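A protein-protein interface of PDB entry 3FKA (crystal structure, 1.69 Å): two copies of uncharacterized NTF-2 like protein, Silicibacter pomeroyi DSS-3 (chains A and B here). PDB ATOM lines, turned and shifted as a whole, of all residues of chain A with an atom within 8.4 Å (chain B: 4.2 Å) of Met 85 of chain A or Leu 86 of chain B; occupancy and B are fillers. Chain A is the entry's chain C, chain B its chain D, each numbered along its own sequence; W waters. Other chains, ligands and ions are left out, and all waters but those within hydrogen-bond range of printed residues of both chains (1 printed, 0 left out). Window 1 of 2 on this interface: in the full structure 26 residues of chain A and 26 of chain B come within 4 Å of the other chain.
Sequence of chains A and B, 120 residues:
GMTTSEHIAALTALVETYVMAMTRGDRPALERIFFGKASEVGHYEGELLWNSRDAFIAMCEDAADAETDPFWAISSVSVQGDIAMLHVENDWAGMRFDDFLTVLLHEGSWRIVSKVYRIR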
ATOM      1  N   LEU A  11       1.098  27.480  11.897  1.00  0.00           N
ATOM      2  CA  LEU A  11       1.554  27.657  13.272  1.00  0.00           C
ATOM      3  C   LEU A  11       0.813  28.819  13.968  1.00  0.00           C
ATOM      4  O   LEU A  11       0.434  28.687  15.105  1.00  0.00           O
ATOM      5  CB  LEU A  11       3.087  27.844  13.303  1.00  0.00           C
ATOM      6  CG  LEU A  11       3.868  26.549  12.956  1.00  0.00           C
ATOM      7  CD1 LEU A  11       5.330  26.825  12.596  1.00  0.00           C
ATOM      8  CD2 LEU A  11       3.774  25.565  14.096  1.00  0.00           C
ATOM      9  N   VAL A  15      -1.897  28.614  17.264  1.00  0.00           N
ATOM     10  CA  VAL A  15      -1.938  29.470  18.461  1.00  0.00           C
ATOM     11  C   VAL A  15      -3.371  29.985  18.702  1.00  0.00           C
ATOM     12  O   VAL A  15      -3.887  29.917  19.817  1.00  0.00           O
ATOM     13  CB  VAL A  15      -0.972  30.660  18.385  1.00  0.00           C
ATOM     14  CG1 VAL A  15      -1.145  31.595  19.604  1.00  0.00           C
ATOM     15  CG2 VAL A  15       0.472  30.192  18.291  1.00  0.00           C
ATOM     16  N   ILE A  74       1.469  36.670  19.737  1.00  0.00           N
ATOM     17  CA  ILE A  74       2.588  35.801  19.380  1.00  0.00           C
ATOM     18  C   ILE A  74       3.822  36.695  19.391  1.00  0.00           C
ATOM     19  O   ILE A  74       3.843  37.721  18.699  1.00  0.00           O
ATOM     20  CB  ILE A  74       2.427  35.170  18.005  1.00  0.00           C
ATOM     21  CG1 ILE A  74       1.175  34.288  17.946  1.00  0.00           C
ATOM     22  CG2 ILE A  74       3.649  34.344  17.668  1.00  0.00           C
ATOM     23  CD1 ILE A  74       0.888  33.742  16.567  1.00  0.00           C
ATOM     24  N   SER A  75       4.801  36.341  20.225  1.00  0.00           N
ATOM     25  CA  SER A  75       6.059  37.075  20.343  1.00  0.00           C
ATOM     26  C   SER A  75       7.087  36.544  19.366  1.00  0.00           C
ATOM     27  O   SER A  75       7.825  37.332  18.815  1.00  0.00           O
ATOM     28  CB  SER A  75       6.614  36.988  21.751  1.00  0.00           C
ATOM     29  OG  SER A  75       5.722  37.620  22.642  1.00  0.00           O
ATOM     30  N   SER A  76       7.165  35.232  19.177  1.00  0.00           N
ATOM     31  CA  SER A  76       8.113  34.674  18.226  1.00  0.00           C
ATOM     32  C   SER A  76       7.685  33.309  17.765  1.00  0.00           C
ATOM     33  O   SER A  76       6.960  32.606  18.478  1.00  0.00           O
ATOM     34  CB  SER A  76       9.553  34.594  18.800  1.00  0.00           C
ATOM     35  OG  SER A  76       9.680  33.610  19.829  1.00  0.00           O
ATOM     36  N   VAL A  77       8.157  32.956  16.574  1.00  0.00           N
ATOM     37  CA  VAL A  77       7.929  31.674  15.926  1.00  0.00           C
ATOM     38  C   VAL A  77       9.265  31.284  15.311  1.00  0.00           C
ATOM     39  O   VAL A  77       9.865  32.099  14.619  1.00  0.00           O
ATOM     40  CB  VAL A  77       6.910  31.739  14.769  1.00  0.00           C
ATOM     41  CG1 VAL A  77       6.728  30.359  14.138  1.00  0.00           C
ATOM     42  CG2 VAL A  77       5.585  32.309  15.236  1.00  0.00           C
ATOM     43  N   SER A  78       9.745  30.072  15.601  1.00  0.00           N
ATOM     44  CA  SER A  78      10.991  29.548  15.072  1.00  0.00           C
ATOM     45  C   SER A  78      10.709  28.195  14.458  1.00  0.00           C
ATOM     46  O   SER A  78       9.986  27.407  15.064  1.00  0.00           O
ATOM     47  CB  SER A  78      12.024  29.407  16.177  1.00  0.00           C
ATOM     48  OG  SER A  78      12.291  30.678  16.746  1.00  0.00           O
ATOM     49  N   VAL A  79      11.310  27.916  13.298  1.00  0.00           N
ATOM     50  CA  VAL A  79      11.100  26.667  12.570  1.00  0.00           C
ATOM     51  C   VAL A  79      12.381  26.080  12.012  1.00  0.00           C
ATOM     52  O   VAL A  79      13.189  26.800  11.428  1.00  0.00           O
ATOM     53  CB  VAL A  79      10.148  26.879  11.352  1.00  0.00           C
ATOM     54  CG1 VAL A  79       9.878  25.566  10.639  1.00  0.00           C
ATOM     55  CG2 VAL A  79       8.844  27.528  11.791  1.00  0.00           C
ATOM     56  N   GLN A  80      12.565  24.778  12.196  1.00  0.00           N
ATOM     57  CA  GLN A  80      13.703  24.059  11.631  1.00  0.00           C
ATOM     58  C   GLN A  80      13.104  22.763  11.141  1.00  0.00           C
ATOM     59  O   GLN A  80      12.716  21.924  11.936  1.00  0.00           O
ATOM     60  CB  GLN A  80      14.817  23.808  12.651  1.00  0.00           C
ATOM     61  CG  GLN A  80      15.561  25.027  13.067  1.00  0.00           C
ATOM     62  CD  GLN A  80      16.447  25.614  11.988  1.00  0.00           C
ATOM     63  OE1 GLN A  80      17.116  24.894  11.239  1.00  0.00           O
ATOM     64  NE2 GLN A  80      16.497  26.932  11.931  1.00  0.00           N
ATOM     65  N   ASP A  82      10.807  20.016  10.451  1.00  0.00           N
ATOM     66  CA  ASP A  82       9.501  19.632  11.017  1.00  0.00           C
ATOM     67  C   ASP A  82       9.323  19.931  12.511  1.00  0.00           C
ATOM     68  O   ASP A  82       8.429  19.370  13.120  1.00  0.00           O
ATOM     69  CB  ASP A  82       9.166  18.144  10.670  1.00  0.00           C
ATOM     70  CG  ASP A  82      10.134  17.126  11.256  1.00  0.00           C
ATOM     71  OD1 ASP A  82      10.969  17.479  12.093  1.00  0.00           O
ATOM     72  OD2 ASP A  82      10.034  15.930  10.875  1.00  0.00           O
ATOM     73  N   ILE A  83      10.167  20.792  13.081  1.00  0.00           N
ATOM     74  CA  ILE A  83      10.027  21.193  14.486  1.00  0.00           C
ATOM     75  C   ILE A  83       9.930  22.706  14.560  1.00  0.00           C
ATOM     76  O   ILE A  83      10.496  23.438  13.727  1.00  0.00           O
ATOM     77  CB  ILE A  83      11.147  20.631  15.412  1.00  0.00           C
ATOM     78  CG1 ILE A  83      12.543  21.132  15.022  1.00  0.00           C
ATOM     79  CG2 ILE A  83      11.053  19.073  15.416  1.00  0.00           C
ATOM     80  CD1 ILE A  83      13.680  20.776  16.024  1.00  0.00           C
ATOM     81  N   ALA A  84       9.197  23.162  15.556  1.00  0.00           N
ATOM     82  CA  ALA A  84       8.986  24.572  15.784  1.00  0.00           C
ATOM     83  C   ALA A  84       8.829  24.919  17.238  1.00  0.00           C
ATOM     84  O   ALA A  84       8.475  24.079  18.046  1.00  0.00           O
ATOM     85  CB  ALA A  84       7.713  25.035  15.034  1.00  0.00           C
ATOM     86  N   MET A  85       9.178  26.153  17.571  1.00  0.00           N
ATOM     87  CA  MET A  85       9.001  26.680  18.928  1.00  0.00           C
ATOM     88  C   MET A  85       8.313  28.019  18.814  1.00  0.00           C
ATOM     89  O   MET A  85       8.641  28.803  17.925  1.00  0.00           O
ATOM     90  CB  MET A  85      10.308  26.760  19.721  1.00  0.00           C
ATOM     91  CG  MET A  85      10.742  25.418  20.248  1.00  0.00           C
ATOM     92  SD  MET A  85      12.078  25.661  21.634  1.00  0.00           S
ATOM     93  CE  MET A  85      13.484  26.445  20.587  1.00  0.00           C
ATOM     94  N   LEU A  86       7.328  28.248  19.686  1.00  0.00           N
ATOM     95  CA  LEU A  86       6.537  29.457  19.686  1.00  0.00           C
ATOM     96  C   LEU A  86       6.534  30.107  21.059  1.00  0.00           C
ATOM     97  O   LEU A  86       6.477  29.402  22.071  1.00  0.00           O
ATOM     98  CB  LEU A  86       5.091  29.094  19.324  1.00  0.00           C
ATOM     99  CG  LEU A  86       4.882  28.145  18.129  1.00  0.00           C
ATOM    100  CD1 LEU A  86       3.402  27.715  17.979  1.00  0.00           C
ATOM    101  CD2 LEU A  86       5.424  28.766  16.859  1.00  0.00           C
ATOM    102  N   HIS A  87       6.586  31.432  21.084  1.00  0.00           N
ATOM    103  CA  HIS A  87       6.499  32.185  22.313  1.00  0.00           C
ATOM    104  C   HIS A  87       5.179  32.941  22.144  1.00  0.00           C
ATOM    105  O   HIS A  87       5.045  33.808  21.270  1.00  0.00           O
ATOM    106  CB  HIS A  87       7.698  33.086  22.580  1.00  0.00           C
ATOM    107  CG  HIS A  87       7.516  34.011  23.743  1.00  0.00           C
ATOM    108  ND1 HIS A  87       8.225  35.184  23.865  1.00  0.00           N
ATOM    109  CD2 HIS A  87       6.643  33.989  24.782  1.00  0.00           C
ATOM    110  CE1 HIS A  87       7.830  35.825  24.954  1.00  0.00           C
ATOM    111  NE2 HIS A  87       6.868  35.124  25.528  1.00  0.00           N
ATOM    112  N   VAL A  88       4.220  32.610  23.006  1.00  0.00           N
ATOM    113  CA  VAL A  88       2.897  33.220  23.022  1.00  0.00           C
ATOM    114  C   VAL A  88       2.623  33.880  24.377  1.00  0.00           C
ATOM    115  O   VAL A  88       2.954  33.312  25.427  1.00  0.00           O
ATOM    116  CB  VAL A  88       1.779  32.179  22.774  1.00  0.00           C
ATOM    117  CG1 VAL A  88       0.365  32.835  22.782  1.00  0.00           C
ATOM    118  CG2 VAL A  88       2.030  31.422  21.472  1.00  0.00           C
ATOM    119  N   ASP A  99       3.985  31.600  27.347  1.00  0.00           N
ATOM    120  CA  ASP A  99       3.952  30.185  26.995  1.00  0.00           C
ATOM    121  C   ASP A  99       5.015  29.928  25.960  1.00  0.00           C
ATOM    122  O   ASP A  99       5.087  30.672  24.970  1.00  0.00           O
ATOM    123  CB  ASP A  99       2.635  29.766  26.320  1.00  0.00           C
ATOM    124  CG  ASP A  99       1.436  29.731  27.260  1.00  0.00           C
ATOM    125  OD1 ASP A  99       1.622  29.603  28.486  1.00  0.00           O
ATOM    126  OD2 ASP A  99       0.287  29.801  26.746  1.00  0.00           O
ATOM    127  N   PHE A 100       5.843  28.917  26.200  1.00  0.00           N
ATOM    128  CA  PHE A 100       6.862  28.472  25.253  1.00  0.00           C
ATOM    129  C   PHE A 100       6.346  27.103  24.820  1.00  0.00           C
ATOM    130  O   PHE A 100       6.336  26.173  25.633  1.00  0.00           O
ATOM    131  CB  PHE A 100       8.264  28.346  25.818  1.00  0.00           C
ATOM    132  CG  PHE A 100       8.963  29.638  26.149  1.00  0.00           C
ATOM    133  CD1 PHE A 100       8.642  30.880  25.583  1.00  0.00           C
ATOM    134  CD2 PHE A 100      10.099  29.571  26.932  1.00  0.00           C
ATOM    135  CE1 PHE A 100       9.393  32.026  25.896  1.00  0.00           C
ATOM    136  CE2 PHE A 100      10.836  30.694  27.221  1.00  0.00           C
ATOM    137  CZ  PHE A 100      10.502  31.917  26.707  1.00  0.00           C
ATOM    138  N   LEU A 101       5.927  27.001  23.553  1.00  0.00           N
ATOM    139  CA  LEU A 101       5.383  25.771  23.000  1.00  0.00           C
ATOM    140  C   LEU A 101       6.368  25.142  22.034  1.00  0.00           C
ATOM    141  O   LEU A 101       6.984  25.864  21.270  1.00  0.00           O
ATOM    142  CB  LEU A 101       4.093  26.065  22.232  1.00  0.00           C
ATOM    143  CG  LEU A 101       3.032  26.953  22.897  1.00  0.00           C
ATOM    144  CD1 LEU A 101       1.812  27.179  21.965  1.00  0.00           C
ATOM    145  CD2 LEU A 101       2.597  26.369  24.194  1.00  0.00           C
ATOM    146  N   THR A 102       6.527  23.822  22.089  1.00  0.00           N
ATOM    147  CA  THR A 102       7.382  23.091  21.148  1.00  0.00           C
ATOM    148  C   THR A 102       6.359  22.289  20.343  1.00  0.00           C
ATOM    149  O   THR A 102       5.453  21.704  20.921  1.00  0.00           O
ATOM    150  CB  THR A 102       8.424  22.221  21.811  1.00  0.00           C
ATOM    151  OG1 THR A 102       9.260  23.043  22.622  1.00  0.00           O
ATOM    152  CG2 THR A 102       9.283  21.561  20.755  1.00  0.00           C
ATOM    153  N   VAL A 103       6.494  22.323  19.021  1.00  0.00           N
ATOM    154  CA  VAL A 103       5.572  21.711  18.089  1.00  0.00           C
ATOM    155  C   VAL A 103       6.287  20.845  17.069  1.00  0.00           C
ATOM    156  O   VAL A 103       7.423  21.137  16.694  1.00  0.00           O
ATOM    157  CB  VAL A 103       4.837  22.861  17.364  1.00  0.00           C
ATOM    158  CG1 VAL A 103       3.569  22.399  16.721  1.00  0.00           C
ATOM    159  CG2 VAL A 103       4.504  24.019  18.363  1.00  0.00           C
ATOM    160  N   LEU A 104       5.605  19.788  16.629  1.00  0.00           N
ATOM    161  CA  LEU A 104       6.132  18.846  15.647  1.00  0.00           C
ATOM    162  C   LEU A 104       5.149  18.660  14.493  1.00  0.00           C
ATOM    163  O   LEU A 104       3.948  18.485  14.741  1.00  0.00           O
ATOM    164  CB  LEU A 104       6.374  17.489  16.288  1.00  0.00           C
ATOM    165  CG  LEU A 104       6.950  16.345  15.420  1.00  0.00           C
ATOM    166  CD1 LEU A 104       8.419  16.608  15.074  1.00  0.00           C
ATOM    167  CD2 LEU A 104       6.819  14.998  16.098  1.00  0.00           C
ATOM    168  N   TRP A 110       0.746  20.209  12.347  1.00  0.00           N
ATOM    169  CA  TRP A 110       1.595  20.668  13.421  1.00  0.00           C
ATOM    170  C   TRP A 110       0.846  20.411  14.717  1.00  0.00           C
ATOM    171  O   TRP A 110      -0.281  20.875  14.851  1.00  0.00           O
ATOM    172  CB  TRP A 110       1.885  22.147  13.320  1.00  0.00           C
ATOM    173  CG  TRP A 110       2.762  22.524  12.211  1.00  0.00           C
ATOM    174  CD1 TRP A 110       2.395  22.939  10.966  1.00  0.00           C
ATOM    175  CD2 TRP A 110       4.188  22.497  12.229  1.00  0.00           C
ATOM    176  NE1 TRP A 110       3.513  23.201  10.221  1.00  0.00           N
ATOM    177  CE2 TRP A 110       4.629  22.933  10.973  1.00  0.00           C
ATOM    178  CE3 TRP A 110       5.145  22.159  13.208  1.00  0.00           C
ATOM    179  CZ2 TRP A 110       5.986  23.045  10.658  1.00  0.00           C
ATOM    180  CZ3 TRP A 110       6.484  22.267  12.892  1.00  0.00           C
ATOM    181  CH2 TRP A 110       6.896  22.702  11.630  1.00  0.00           C
ATOM    182  N   SER A 114       4.982  20.061  23.820  1.00  0.00           N
ATOM    183  CA  SER A 114       5.101  20.556  25.176  1.00  0.00           C
ATOM    184  C   SER A 114       4.729  22.018  25.247  1.00  0.00           C
ATOM    185  O   SER A 114       4.853  22.734  24.261  1.00  0.00           O
ATOM    186  CB  SER A 114       6.524  20.371  25.722  1.00  0.00           C
ATOM    187  OG  SER A 114       7.450  21.218  25.082  1.00  0.00           O
ATOM    188  N   VAL A 116       5.496  25.022  28.122  1.00  0.00           N
ATOM    189  CA  VAL A 116       6.136  25.416  29.372  1.00  0.00           C
ATOM    190  C   VAL A 116       5.728  26.876  29.577  1.00  0.00           C
ATOM    191  O   VAL A 116       5.695  27.637  28.610  1.00  0.00           O
ATOM    192  CB  VAL A 116       7.674  25.139  29.365  1.00  0.00           C
ATOM    193  CG1 VAL A 116       8.367  25.741  28.151  1.00  0.00           C
ATOM    194  CG2 VAL A 116       8.314  25.626  30.642  1.00  0.00           C
ATOM    195  N   LEU B  11      22.699  28.640  31.182  1.00  0.00           N
ATOM    196  CA  LEU B  11      22.088  27.906  30.078  1.00  0.00           C
ATOM    197  C   LEU B  11      23.167  27.475  29.061  1.00  0.00           C
ATOM    198  O   LEU B  11      23.072  26.396  28.479  1.00  0.00           O
ATOM    199  CB  LEU B  11      20.989  28.750  29.418  1.00  0.00           C
ATOM    200  CG  LEU B  11      19.710  28.871  30.285  1.00  0.00           C
ATOM    201  CD1 LEU B  11      18.845  30.079  29.871  1.00  0.00           C
ATOM    202  CD2 LEU B  11      18.915  27.562  30.286  1.00  0.00           C
ATOM    203  N   VAL B  15      24.176  23.550  28.029  1.00  0.00           N
ATOM    204  CA  VAL B  15      24.341  23.008  26.671  1.00  0.00           C
ATOM    205  C   VAL B  15      25.684  22.273  26.541  1.00  0.00           C
ATOM    206  O   VAL B  15      25.743  21.162  25.989  1.00  0.00           O
ATOM    207  CB  VAL B  15      24.211  24.090  25.569  1.00  0.00           C
ATOM    208  CG1 VAL B  15      24.539  23.504  24.181  1.00  0.00           C
ATOM    209  CG2 VAL B  15      22.807  24.685  25.597  1.00  0.00           C
ATOM    210  N   SER B  76      20.383  29.750  19.316  1.00  0.00           N
ATOM    211  CA  SER B  76      19.473  30.701  19.927  1.00  0.00           C
ATOM    212  C   SER B  76      19.173  30.358  21.387  1.00  0.00           C
ATOM    213  O   SER B  76      19.144  29.177  21.756  1.00  0.00           O
ATOM    214  CB  SER B  76      18.178  30.783  19.116  1.00  0.00           C
ATOM    215  OG  SER B  76      17.317  31.785  19.610  1.00  0.00           O
ATOM    216  N   VAL B  77      18.960  31.389  22.210  1.00  0.00           N
ATOM    217  CA  VAL B  77      18.623  31.261  23.616  1.00  0.00           C
ATOM    218  C   VAL B  77      17.570  32.333  23.888  1.00  0.00           C
ATOM    219  O   VAL B  77      17.805  33.481  23.554  1.00  0.00           O
ATOM    220  CB  VAL B  77      19.817  31.537  24.552  1.00  0.00           C
ATOM    221  CG1 VAL B  77      19.402  31.430  26.037  1.00  0.00           C
ATOM    222  CG2 VAL B  77      20.978  30.600  24.257  1.00  0.00           C
ATOM    223  N   ALA B  84      13.006  28.998  29.633  1.00  0.00           N
ATOM    224  CA  ALA B  84      13.870  29.280  28.503  1.00  0.00           C
ATOM    225  C   ALA B  84      13.698  28.310  27.370  1.00  0.00           C
ATOM    226  O   ALA B  84      13.185  27.192  27.560  1.00  0.00           O
ATOM    227  CB  ALA B  84      15.374  29.255  28.932  1.00  0.00           C
ATOM    228  N   MET B  85      14.063  28.747  26.169  1.00  0.00           N
ATOM    229  CA  MET B  85      14.082  27.878  24.986  1.00  0.00           C
ATOM    230  C   MET B  85      15.449  28.051  24.329  1.00  0.00           C
ATOM    231  O   MET B  85      15.976  29.162  24.227  1.00  0.00           O
ATOM    232  CB  MET B  85      12.908  28.053  24.004  1.00  0.00           C
ATOM    233  CG  MET B  85      11.671  27.250  24.435  1.00  0.00           C
ATOM    234  SD  MET B  85      10.305  27.074  23.051  1.00  0.00           S
ATOM    235  CE  MET B  85       9.947  28.937  22.881  1.00  0.00           C
ATOM    236  N   LEU B  86      15.999  26.925  23.891  1.00  0.00           N
ATOM    237  CA  LEU B  86      17.308  26.877  23.281  1.00  0.00           C
ATOM    238  C   LEU B  86      17.266  26.131  21.970  1.00  0.00           C
ATOM    239  O   LEU B  86      16.506  25.169  21.827  1.00  0.00           O
ATOM    240  CB  LEU B  86      18.301  26.117  24.174  1.00  0.00           C
ATOM    241  CG  LEU B  86      18.886  26.679  25.474  1.00  0.00           C
ATOM    242  CD1 LEU B  86      19.992  27.677  25.170  1.00  0.00           C
ATOM    243  CD2 LEU B  86      17.796  27.262  26.361  1.00  0.00           C
ATOM    244  N   HIS B  87      18.056  26.612  21.007  1.00  0.00           N
ATOM    245  CA  HIS B  87      18.198  25.986  19.710  1.00  0.00           C
ATOM    246  C   HIS B  87      19.678  25.620  19.694  1.00  0.00           C
ATOM    247  O   HIS B  87      20.556  26.498  19.724  1.00  0.00           O
ATOM    248  CB  HIS B  87      17.801  26.852  18.521  1.00  0.00           C
ATOM    249  CG  HIS B  87      18.117  26.239  17.197  1.00  0.00           C
ATOM    250  ND1 HIS B  87      18.244  26.995  16.053  1.00  0.00           N
ATOM    251  CD2 HIS B  87      18.446  24.967  16.851  1.00  0.00           C
ATOM    252  CE1 HIS B  87      18.586  26.201  15.050  1.00  0.00           C
ATOM    253  NE2 HIS B  87      18.724  24.971  15.511  1.00  0.00           N
ATOM    254  N   VAL B  88      19.938  24.319  19.675  1.00  0.00           N
ATOM    255  CA  VAL B  88      21.275  23.801  19.656  1.00  0.00           C
ATOM    256  C   VAL B  88      21.487  22.985  18.395  1.00  0.00           C
ATOM    257  O   VAL B  88      20.622  22.162  18.046  1.00  0.00           O
ATOM    258  CB  VAL B  88      21.542  22.912  20.880  1.00  0.00           C
ATOM    259  CG1 VAL B  88      22.969  22.269  20.834  1.00  0.00           C
ATOM    260  CG2 VAL B  88      21.342  23.711  22.182  1.00  0.00           C
ATOM    261  N   ASP B  99      18.274  20.674  17.781  1.00  0.00           N
ATOM    262  CA  ASP B  99      17.572  20.349  19.005  1.00  0.00           C
ATOM    263  C   ASP B  99      16.871  21.608  19.496  1.00  0.00           C
ATOM    264  O   ASP B  99      17.503  22.648  19.606  1.00  0.00           O
ATOM    265  CB  ASP B  99      18.516  19.909  20.126  1.00  0.00           C
ATOM    266  CG  ASP B  99      19.241  18.593  19.845  1.00  0.00           C
ATOM    267  OD1 ASP B  99      19.126  18.023  18.738  1.00  0.00           O
ATOM    268  OD2 ASP B  99      19.954  18.133  20.776  1.00  0.00           O
ATOM    269  N   PHE B 100      15.586  21.506  19.774  1.00  0.00           N
ATOM    270  CA  PHE B 100      14.805  22.602  20.341  1.00  0.00           C
ATOM    271  C   PHE B 100      14.497  22.152  21.766  1.00  0.00           C
ATOM    272  O   PHE B 100      13.688  21.204  21.996  1.00  0.00           O
ATOM    273  CB  PHE B 100      13.519  22.929  19.599  1.00  0.00           C
ATOM    274  CG  PHE B 100      13.687  23.677  18.308  1.00  0.00           C
ATOM    275  CD1 PHE B 100      14.841  24.404  17.964  1.00  0.00           C
ATOM    276  CD2 PHE B 100      12.570  23.855  17.518  1.00  0.00           C
ATOM    277  CE1 PHE B 100      14.871  25.142  16.793  1.00  0.00           C
ATOM    278  CE2 PHE B 100      12.607  24.599  16.370  1.00  0.00           C
ATOM    279  CZ  PHE B 100      13.746  25.247  16.004  1.00  0.00           C
ATOM    280  N   LEU B 101      15.120  22.821  22.732  1.00  0.00           N
ATOM    281  CA  LEU B 101      14.964  22.470  24.131  1.00  0.00           C
ATOM    282  C   LEU B 101      14.224  23.513  24.930  1.00  0.00           C
ATOM    283  O   LEU B 101      14.468  24.693  24.709  1.00  0.00           O
ATOM    284  CB  LEU B 101      16.341  22.356  24.784  1.00  0.00           C
ATOM    285  CG  LEU B 101      17.442  21.507  24.158  1.00  0.00           C
ATOM    286  CD1 LEU B 101      18.752  21.662  24.948  1.00  0.00           C
ATOM    287  CD2 LEU B 101      17.023  20.077  24.085  1.00  0.00           C
ATOM    288  N   VAL B 103      13.437  24.684  28.854  1.00  0.00           N
ATOM    289  CA  VAL B 103      14.052  24.520  30.133  1.00  0.00           C
ATOM    290  C   VAL B 103      13.345  25.328  31.223  1.00  0.00           C
ATOM    291  O   VAL B 103      12.763  26.364  30.940  1.00  0.00           O
ATOM    292  CB  VAL B 103      15.534  25.006  29.964  1.00  0.00           C
ATOM    293  CG1 VAL B 103      16.420  24.440  31.041  1.00  0.00           C
ATOM    294  CG2 VAL B 103      16.140  24.597  28.585  1.00  0.00           C
HETATM  295  O   HOH W   1      11.345  21.433  23.448  1.00  0.00           O
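O of Leu 86 of chain A lies within hydrogen-bond range of N of Leu 101 of chain A (2.9 Å). N of Ser 78 of chain A lies within hydrogen-bond range of O of Met 85 of chain A (2.9 Å). O of Val 116 of chain A lies within hydrogen-bond range of N of Phe 100 of chain A (2.7 Å). The backbone carbonyl oxygen (O) of Ser 76 of chain B sits at hydrogen-bond distance from the backbone NH (N) of His 87 of chain B. The backbone NH (N) of Val 103 of chain B lies within hydrogen-bond range of the backbone carbonyl oxygen (O) of Ala 84 of chain B. The backbone carbonyl oxygen of Ala 84 of chain A is in hydrogen-bond range of the backbone NH of Val 103 of chain A, at 2.8 Å.
Gln 80 of chain A touches His 87 of chain B (CD to CE1, 3.8 Å). Gln 80 of chain A touches Phe 100 of chain B (CG to CZ, 3.5 Å). Ile 83 of chain A touches Phe 100 of chain B (O to CE2, 3.6 Å). Ala 84 of chain A touches Phe 100 of chain B (CA to CE2, 3.7 Å). CE of Met 85 of chain A touches O of Leu 86 of chain B, 3.5 Å away. Met 85 of chain A touches Phe 100 of chain B. Leu 86 of chain A touches Met 85 of chain B. Phe 100 of chain A touches Ala 84 of chain B (CE2 to CA, 3.6 Å). CB of Phe 100 of chain A touches CE of Met 85 of chain B (3.4 Å). Leu 101 of chain A touches Met 85 of chain B.
Of the 13 printed residues of chain B, 5 touch a printed residue of chain A. Hydrophobic or aromatic side chains of chain B within 4 Å of the printed part of chain A: Met 85, His 87 and Phe 100. Of the 25 printed residues of chain A, 7 touch a printed residue of chain B. Among the printed residues, no Asp or Glu carboxylate lies within 4 Å of a Lys or Arg side-chain nitrogen of the other chain.
Printed residues of chain B within 4 Å of Ile 83 of chain A: Phe 100. Of the printed residues of chain B, Met 85 of chain A touches Met 85, Leu 86 and Phe 100. Printed residues of chain A within 4 Å of Leu 86 of chain B: Met 85. Printed residues of chain A within 4 Å of Phe 100 of chain B: Gln 80, Ile 83, Ala 84 and Met 85. The nearest printed residue of chain B that does not touch Met 85 of chain A is Leu 101 of chain B (4.01 Å). The nearest printed residue of chain A that does not touch Leu 86 of chain B is Phe 100 of chain A (7.1 Å). The nearest printed residue of chain A that does not touch Phe 100 of chain B is Ser 78 of chain A (4.1 Å).
Water W1 lies within hydrogen-bond range of OG1 of Thr 102 of chain A and O of Phe 100 of chain B.
Met 85 of chain A touches its own counterpart, Met 85 of chain B. Met 85 of chain A touches Leu 86 of chain B, and with the chains exchanged Leu 86 of chain A touches Met 85 of chain B. Met 85 of chain A touches Phe 100 of chain B, and with the chains exchanged Phe 100 of chain A touches Met 85 of chain B. Leu 101 of chain A touches Met 85 of chain B, but with the chains exchanged Met 85 of chain A does not touch Leu 101 of chain B (4.01 Å). 13 positions are printed for both chains. Of the 11 pairs that touch across the chains among the printed residues, 7 have their exchanged pair printed and touching as well.
SD of Met 85 of chain B sits close to SD of Met 85 of chain A (2.7 Å).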
